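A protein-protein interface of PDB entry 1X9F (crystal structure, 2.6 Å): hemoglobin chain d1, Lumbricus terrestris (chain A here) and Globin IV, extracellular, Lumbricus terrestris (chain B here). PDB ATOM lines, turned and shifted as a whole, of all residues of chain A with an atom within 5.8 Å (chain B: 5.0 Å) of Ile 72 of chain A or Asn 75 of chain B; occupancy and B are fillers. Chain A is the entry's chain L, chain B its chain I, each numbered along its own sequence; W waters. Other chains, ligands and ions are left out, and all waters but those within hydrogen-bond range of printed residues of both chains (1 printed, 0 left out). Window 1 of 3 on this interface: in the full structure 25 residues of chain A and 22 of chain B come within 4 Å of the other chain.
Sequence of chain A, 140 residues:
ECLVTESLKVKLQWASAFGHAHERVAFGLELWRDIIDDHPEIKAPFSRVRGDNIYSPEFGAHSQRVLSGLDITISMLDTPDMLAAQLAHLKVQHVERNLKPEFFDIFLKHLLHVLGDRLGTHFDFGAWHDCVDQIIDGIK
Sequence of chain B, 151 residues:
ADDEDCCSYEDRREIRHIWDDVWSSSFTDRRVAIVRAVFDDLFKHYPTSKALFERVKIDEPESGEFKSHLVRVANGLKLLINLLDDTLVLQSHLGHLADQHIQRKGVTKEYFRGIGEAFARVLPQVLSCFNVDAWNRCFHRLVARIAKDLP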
ATOM      1  N   LEU A  67     -24.760  11.789 -11.167  1.00  0.00           N
ATOM      2  CA  LEU A  67     -23.502  11.799 -11.905  1.00  0.00           C
ATOM      3  C   LEU A  67     -22.802  13.138 -11.748  1.00  0.00           C
ATOM      4  O   LEU A  67     -21.577  13.193 -11.620  1.00  0.00           O
ATOM      5  CB  LEU A  67     -23.704  11.469 -13.391  1.00  0.00           C
ATOM      6  CG  LEU A  67     -23.851  10.005 -13.841  1.00  0.00           C
ATOM      7  CD1 LEU A  67     -22.720   9.118 -13.323  1.00  0.00           C
ATOM      8  CD2 LEU A  67     -25.197   9.417 -13.440  1.00  0.00           C
ATOM      9  N   SER A  68     -23.575  14.217 -11.745  1.00  0.00           N
ATOM     10  CA  SER A  68     -22.995  15.537 -11.565  1.00  0.00           C
ATOM     11  C   SER A  68     -22.373  15.659 -10.168  1.00  0.00           C
ATOM     12  O   SER A  68     -21.337  16.306  -9.997  1.00  0.00           O
ATOM     13  CB  SER A  68     -24.049  16.621 -11.817  1.00  0.00           C
ATOM     14  OG  SER A  68     -23.484  17.921 -11.696  1.00  0.00           O
ATOM     15  N   GLY A  69     -23.006  15.021  -9.184  1.00  0.00           N
ATOM     16  CA  GLY A  69     -22.481  14.947  -7.823  1.00  0.00           C
ATOM     17  C   GLY A  69     -21.194  14.146  -7.751  1.00  0.00           C
ATOM     18  O   GLY A  69     -20.233  14.568  -7.103  1.00  0.00           O
ATOM     19  N   LEU A  70     -21.178  12.992  -8.414  1.00  0.00           N
ATOM     20  CA  LEU A  70     -19.967  12.196  -8.517  1.00  0.00           C
ATOM     21  C   LEU A  70     -18.864  13.040  -9.140  1.00  0.00           C
ATOM     22  O   LEU A  70     -17.698  12.950  -8.741  1.00  0.00           O
ATOM     23  CB  LEU A  70     -20.213  10.968  -9.393  1.00  0.00           C
ATOM     24  CG  LEU A  70     -19.753   9.596  -8.890  1.00  0.00           C
ATOM     25  CD1 LEU A  70     -19.732   8.630 -10.063  1.00  0.00           C
ATOM     26  CD2 LEU A  70     -18.390   9.631  -8.199  1.00  0.00           C
ATOM     27  N   ASP A  71     -19.245  13.861 -10.115  1.00  0.00           N
ATOM     28  CA  ASP A  71     -18.278  14.669 -10.833  1.00  0.00           C
ATOM     29  C   ASP A  71     -17.624  15.682  -9.902  1.00  0.00           C
ATOM     30  O   ASP A  71     -16.401  15.880  -9.944  1.00  0.00           O
ATOM     31  CB  ASP A  71     -18.934  15.375 -12.009  1.00  0.00           C
ATOM     32  CG  ASP A  71     -17.926  16.062 -12.873  1.00  0.00           C
ATOM     33  OD1 ASP A  71     -17.820  17.305 -12.797  1.00  0.00           O
ATOM     34  OD2 ASP A  71     -17.160  15.435 -13.634  1.00  0.00           O
ATOM     35  N   ILE A  72     -18.446  16.305  -9.055  1.00  0.00           N
ATOM     36  CA  ILE A  72     -17.966  17.257  -8.061  1.00  0.00           C
ATOM     37  C   ILE A  72     -16.921  16.601  -7.166  1.00  0.00           C
ATOM     38  O   ILE A  72     -15.831  17.153  -6.983  1.00  0.00           O
ATOM     39  CB  ILE A  72     -19.129  17.845  -7.218  1.00  0.00           C
ATOM     40  CG1 ILE A  72     -20.069  18.676  -8.097  1.00  0.00           C
ATOM     41  CG2 ILE A  72     -18.573  18.714  -6.084  1.00  0.00           C
ATOM     42  CD1 ILE A  72     -21.380  19.085  -7.425  1.00  0.00           C
ATOM     43  N   THR A  73     -17.233  15.418  -6.635  1.00  0.00           N
ATOM     44  CA  THR A  73     -16.320  14.762  -5.699  1.00  0.00           C
ATOM     45  C   THR A  73     -15.026  14.312  -6.367  1.00  0.00           C
ATOM     46  O   THR A  73     -13.951  14.439  -5.773  1.00  0.00           O
ATOM     47  CB  THR A  73     -16.984  13.579  -4.968  1.00  0.00           C
ATOM     48  OG1 THR A  73     -17.424  12.607  -5.923  1.00  0.00           O
ATOM     49  CG2 THR A  73     -18.264  14.016  -4.275  1.00  0.00           C
ATOM     50  N   ILE A  74     -15.123  13.794  -7.592  1.00  0.00           N
ATOM     51  CA  ILE A  74     -13.925  13.389  -8.324  1.00  0.00           C
ATOM     52  C   ILE A  74     -13.012  14.593  -8.569  1.00  0.00           C
ATOM     53  O   ILE A  74     -11.802  14.514  -8.354  1.00  0.00           O
ATOM     54  CB  ILE A  74     -14.267  12.631  -9.628  1.00  0.00           C
ATOM     55  CG1 ILE A  74     -14.892  11.267  -9.293  1.00  0.00           C
ATOM     56  CG2 ILE A  74     -13.013  12.439 -10.488  1.00  0.00           C
ATOM     57  CD1 ILE A  74     -15.427  10.508 -10.509  1.00  0.00           C
ATOM     58  N   SER A  75     -13.588  15.717  -8.978  1.00  0.00           N
ATOM     59  CA  SER A  75     -12.795  16.927  -9.189  1.00  0.00           C
ATOM     60  C   SER A  75     -12.235  17.527  -7.889  1.00  0.00           C
ATOM     61  O   SER A  75     -11.404  18.438  -7.921  1.00  0.00           O
ATOM     62  CB  SER A  75     -13.600  17.967  -9.959  1.00  0.00           C
ATOM     63  OG  SER A  75     -14.712  18.395  -9.195  1.00  0.00           O
ATOM     64  N   MET A  76     -12.676  17.005  -6.749  1.00  0.00           N
ATOM     65  CA  MET A  76     -12.208  17.485  -5.454  1.00  0.00           C
ATOM     66  C   MET A  76     -11.219  16.544  -4.761  1.00  0.00           C
ATOM     67  O   MET A  76     -10.765  16.839  -3.653  1.00  0.00           O
ATOM     68  CB  MET A  76     -13.395  17.746  -4.528  1.00  0.00           C
ATOM     69  CG  MET A  76     -14.134  19.040  -4.799  1.00  0.00           C
ATOM     70  SD  MET A  76     -15.505  19.187  -3.645  1.00  0.00           S
ATOM     71  CE  MET A  76     -16.214  20.738  -4.186  1.00  0.00           C
ATOM     72  N   LEU A  77     -10.884  15.425  -5.401  1.00  0.00           N
ATOM     73  CA  LEU A  77      -9.999  14.416  -4.798  1.00  0.00           C
ATOM     74  C   LEU A  77      -8.667  14.974  -4.300  1.00  0.00           C
ATOM     75  O   LEU A  77      -8.024  14.379  -3.433  1.00  0.00           O
ATOM     76  CB  LEU A  77      -9.726  13.299  -5.801  1.00  0.00           C
ATOM     77  CG  LEU A  77     -10.405  11.927  -5.717  1.00  0.00           C
ATOM     78  CD1 LEU A  77     -11.456  11.793  -4.602  1.00  0.00           C
ATOM     79  CD2 LEU A  77     -11.000  11.593  -7.084  1.00  0.00           C
ATOM     80  N   GLN A  86     -17.926  18.924   0.898  1.00  0.00           N
ATOM     81  CA  GLN A  86     -18.825  18.345  -0.088  1.00  0.00           C
ATOM     82  C   GLN A  86     -19.414  17.004   0.348  1.00  0.00           C
ATOM     83  O   GLN A  86     -20.623  16.779   0.206  1.00  0.00           O
ATOM     84  CB  GLN A  86     -18.118  18.205  -1.434  1.00  0.00           C
ATOM     85  CG  GLN A  86     -19.003  17.643  -2.539  1.00  0.00           C
ATOM     86  CD  GLN A  86     -20.205  18.529  -2.856  1.00  0.00           C
ATOM     87  OE1 GLN A  86     -20.193  19.741  -2.605  1.00  0.00           O
ATOM     88  NE2 GLN A  86     -21.244  17.924  -3.425  1.00  0.00           N
ATOM     89  N   TRP B  23     -15.461  25.245 -19.104  1.00  0.00           N
ATOM     90  CA  TRP B  23     -15.458  24.051 -18.263  1.00  0.00           C
ATOM     91  C   TRP B  23     -14.390  23.061 -18.699  1.00  0.00           C
ATOM     92  O   TRP B  23     -14.688  21.998 -19.261  1.00  0.00           O
ATOM     93  CB  TRP B  23     -16.831  23.376 -18.261  1.00  0.00           C
ATOM     94  CG  TRP B  23     -17.035  22.427 -17.112  1.00  0.00           C
ATOM     95  CD1 TRP B  23     -16.698  21.102 -17.061  1.00  0.00           C
ATOM     96  CD2 TRP B  23     -17.623  22.736 -15.845  1.00  0.00           C
ATOM     97  NE1 TRP B  23     -17.050  20.568 -15.844  1.00  0.00           N
ATOM     98  CE2 TRP B  23     -17.620  21.548 -15.077  1.00  0.00           C
ATOM     99  CE3 TRP B  23     -18.160  23.899 -15.278  1.00  0.00           C
ATOM    100  CZ2 TRP B  23     -18.131  21.492 -13.780  1.00  0.00           C
ATOM    101  CZ3 TRP B  23     -18.663  23.842 -13.990  1.00  0.00           C
ATOM    102  CH2 TRP B  23     -18.645  22.645 -13.255  1.00  0.00           C
ATOM    103  N   ARG B  31     -13.165  26.493 -12.286  1.00  0.00           N
ATOM    104  CA  ARG B  31     -14.596  26.607 -12.002  1.00  0.00           C
ATOM    105  C   ARG B  31     -14.840  27.211 -10.608  1.00  0.00           C
ATOM    106  O   ARG B  31     -15.914  27.971 -10.471  1.00  0.00           O
ATOM    107  CB  ARG B  31     -15.335  25.293 -12.216  1.00  0.00           C
ATOM    108  CG  ARG B  31     -15.298  24.334 -11.070  1.00  0.00           C
ATOM    109  CD  ARG B  31     -15.925  23.002 -11.424  1.00  0.00           C
ATOM    110  NE  ARG B  31     -14.915  22.121 -12.007  1.00  0.00           N
ATOM    111  CZ  ARG B  31     -15.046  20.808 -12.132  1.00  0.00           C
ATOM    112  NH1 ARG B  31     -16.165  20.201 -11.732  1.00  0.00           N
ATOM    113  NH2 ARG B  31     -14.059  20.096 -12.664  1.00  0.00           N
ATOM    114  N   VAL B  71     -18.507  25.474  -6.352  1.00  0.00           N
ATOM    115  CA  VAL B  71     -18.408  24.340  -7.256  1.00  0.00           C
ATOM    116  C   VAL B  71     -19.783  23.720  -7.471  1.00  0.00           C
ATOM    117  O   VAL B  71     -20.096  23.287  -8.579  1.00  0.00           O
ATOM    118  CB  VAL B  71     -17.387  23.282  -6.754  1.00  0.00           C
ATOM    119  CG1 VAL B  71     -17.430  22.011  -7.605  1.00  0.00           C
ATOM    120  CG2 VAL B  71     -15.991  23.872  -6.744  1.00  0.00           C
ATOM    121  N   ARG B  72     -20.613  23.692  -6.428  1.00  0.00           N
ATOM    122  CA  ARG B  72     -21.947  23.102  -6.571  1.00  0.00           C
ATOM    123  C   ARG B  72     -22.764  23.875  -7.595  1.00  0.00           C
ATOM    124  O   ARG B  72     -23.520  23.292  -8.378  1.00  0.00           O
ATOM    125  CB  ARG B  72     -22.679  23.028  -5.230  1.00  0.00           C
ATOM    126  CG  ARG B  72     -22.307  21.806  -4.396  1.00  0.00           C
ATOM    127  CD  ARG B  72     -23.246  21.536  -3.220  1.00  0.00           C
ATOM    128  NE  ARG B  72     -23.242  22.622  -2.240  1.00  0.00           N
ATOM    129  CZ  ARG B  72     -22.335  22.769  -1.282  1.00  0.00           C
ATOM    130  NH1 ARG B  72     -21.338  21.900  -1.151  1.00  0.00           N
ATOM    131  NH2 ARG B  72     -22.424  23.792  -0.444  1.00  0.00           N
ATOM    132  N   VAL B  73     -22.575  25.189  -7.594  1.00  0.00           N
ATOM    133  CA  VAL B  73     -23.224  26.091  -8.533  1.00  0.00           C
ATOM    134  C   VAL B  73     -22.646  25.885  -9.917  1.00  0.00           C
ATOM    135  O   VAL B  73     -23.387  25.774 -10.891  1.00  0.00           O
ATOM    136  CB  VAL B  73     -22.949  27.535  -8.147  1.00  0.00           C
ATOM    137  CG1 VAL B  73     -23.567  28.510  -9.169  1.00  0.00           C
ATOM    138  CG2 VAL B  73     -23.440  27.786  -6.743  1.00  0.00           C
ATOM    139  N   ALA B  74     -21.318  25.869  -9.994  1.00  0.00           N
ATOM    140  CA  ALA B  74     -20.627  25.566 -11.231  1.00  0.00           C
ATOM    141  C   ALA B  74     -21.164  24.251 -11.825  1.00  0.00           C
ATOM    142  O   ALA B  74     -21.617  24.227 -12.977  1.00  0.00           O
ATOM    143  CB  ALA B  74     -19.127  25.506 -11.000  1.00  0.00           C
ATOM    144  N   ASN B  75     -21.149  23.174 -11.036  1.00  0.00           N
ATOM    145  CA  ASN B  75     -21.636  21.879 -11.526  1.00  0.00           C
ATOM    146  C   ASN B  75     -23.128  21.848 -11.821  1.00  0.00           C
ATOM    147  O   ASN B  75     -23.573  21.075 -12.672  1.00  0.00           O
ATOM    148  CB  ASN B  75     -21.242  20.725 -10.602  1.00  0.00           C
ATOM    149  CG  ASN B  75     -19.869  20.169 -10.928  1.00  0.00           C
ATOM    150  OD1 ASN B  75     -18.850  20.816 -10.681  1.00  0.00           O
ATOM    151  ND2 ASN B  75     -19.832  18.959 -11.481  1.00  0.00           N
ATOM    152  N   GLY B  76     -23.897  22.685 -11.127  1.00  0.00           N
ATOM    153  CA  GLY B  76     -25.335  22.796 -11.401  1.00  0.00           C
ATOM    154  C   GLY B  76     -25.570  23.403 -12.772  1.00  0.00           C
ATOM    155  O   GLY B  76     -26.486  23.004 -13.499  1.00  0.00           O
ATOM    156  N   LEU B  77     -24.722  24.370 -13.116  1.00  0.00           N
ATOM    157  CA  LEU B  77     -24.795  25.033 -14.405  1.00  0.00           C
ATOM    158  C   LEU B  77     -24.316  24.094 -15.515  1.00  0.00           C
ATOM    159  O   LEU B  77     -24.941  24.003 -16.576  1.00  0.00           O
ATOM    160  CB  LEU B  77     -23.998  26.341 -14.388  1.00  0.00           C
ATOM    161  CG  LEU B  77     -24.127  27.195 -15.659  1.00  0.00           C
ATOM    162  CD1 LEU B  77     -25.583  27.468 -16.036  1.00  0.00           C
ATOM    163  CD2 LEU B  77     -23.376  28.486 -15.489  1.00  0.00           C
ATOM    164  N   LYS B  78     -23.218  23.386 -15.240  1.00  0.00           N
ATOM    165  CA  LYS B  78     -22.682  22.351 -16.117  1.00  0.00           C
ATOM    166  C   LYS B  78     -23.749  21.294 -16.358  1.00  0.00           C
ATOM    167  O   LYS B  78     -23.902  20.793 -17.479  1.00  0.00           O
ATOM    168  CB  LYS B  78     -21.438  21.720 -15.467  1.00  0.00           C
ATOM    169  CG  LYS B  78     -20.924  20.435 -16.131  1.00  0.00           C
ATOM    170  CD  LYS B  78     -20.540  20.754 -17.563  1.00  0.00           C
ATOM    171  CE  LYS B  78     -19.480  19.808 -18.074  1.00  0.00           C
ATOM    172  NZ  LYS B  78     -18.837  20.407 -19.414  1.00  0.00           N
ATOM    173  N   LEU B  79     -24.489  20.960 -15.300  1.00  0.00           N
ATOM    174  CA  LEU B  79     -25.586  20.012 -15.422  1.00  0.00           C
ATOM    175  C   LEU B  79     -26.607  20.519 -16.435  1.00  0.00           C
ATOM    176  O   LEU B  79     -27.021  19.777 -17.328  1.00  0.00           O
ATOM    177  CB  LEU B  79     -26.270  19.764 -14.075  1.00  0.00           C
ATOM    178  CG  LEU B  79     -26.955  18.406 -13.851  1.00  0.00           C
ATOM    179  CD1 LEU B  79     -28.114  18.581 -12.892  1.00  0.00           C
ATOM    180  CD2 LEU B  79     -27.462  17.739 -15.118  1.00  0.00           C
HETATM  181  O   HOH W   1     -14.528  17.863 -13.630  1.00  0.00           O
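Water W1 bridges NH2 of Arg 31 of chain B (2.5 Å) and OD1 of Asp 71 of chain A (3.4 Å).
The side-chain amide oxygen (OD1) of Asn 75 of chain B is in hydrogen-bond range of the guanidinium group (NH1) of Arg 31 of chain B (2.9 Å). The backbone carbonyl oxygen (O) of Val 71 of chain B lies close to the side-chain amide oxygen (OD1) of Asn 75 of chain B (3.5 Å). The side-chain hydroxyl (OG) of Ser 75 of chain A sits at hydrogen-bond distance from the backbone carbonyl oxygen (O) of Asp 71 of chain A (3.1 Å). The side-chain hydroxyl (OG) of Ser 75 of chain A lies within hydrogen-bond range of the backbone carbonyl oxygen (O) of Ile 72 of chain A, at 2.8 Å.
Asn 75 of chain B touches three residues of chain A. Printed residues of chain B within 4 Å of Asp 71 of chain A: Arg 31 (3.5 Å) and Asn 75 (2.9 Å). Of the printed residues of chain A, Leu 79 of chain B touches Ser 68. The nearest residue of chain A that does not touch Asn 75 of chain B is Ser 75 of chain A (5.0 Å).
Leu 79 of chain B touches Ser 68 of chain A. Val 71 of chain B touches Ile 72 of chain A (CG1 to CG2, 3.8 Å). Ile 72 of chain A touches Asn 75 of chain B (CG1 to CG, 3.2 Å). Val 71 of chain B touches Met 76 of chain A (CB to CE, 3.8 Å).
Hydrophobic or aromatic side chains of chain B within 4 Å of the printed part of chain A: Val 71 and Leu 79. Of the 12 printed residues of chain A, 6 touch a printed residue of chain B. Printed residues of chain A that touch a printed residue of chain B: Ser 68, Asp 71, Ile 72, Ser 75, Met 76 and Gln 86. Hydrophobic or aromatic side chains of chain A within 4 Å of the printed part of chain B: Ile 72 and Met 76.
The guanidinium group (NH1) of Arg 31 of chain B is in salt-bridge range of the side-chain carboxylate (OD1) of Asp 71 of chain A, 3.5 Å away. NH1 of Arg 31 of chain B sits at hydrogen-bond distance from OG of Ser 75 of chain A (3.4 Å). The side-chain amide oxygen of Gln 86 of chain A sits at hydrogen-bond distance from the guanidinium group of Arg 72 of chain B (2.8 Å). O of Asn 75 of chain B lies within hydrogen-bond range of OG of Ser 68 of chain A, at 3.3 Å. ND2 of Asn 75 of chain B lies within hydrogen-bond range of OD1 of Asp 71 of chain A.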
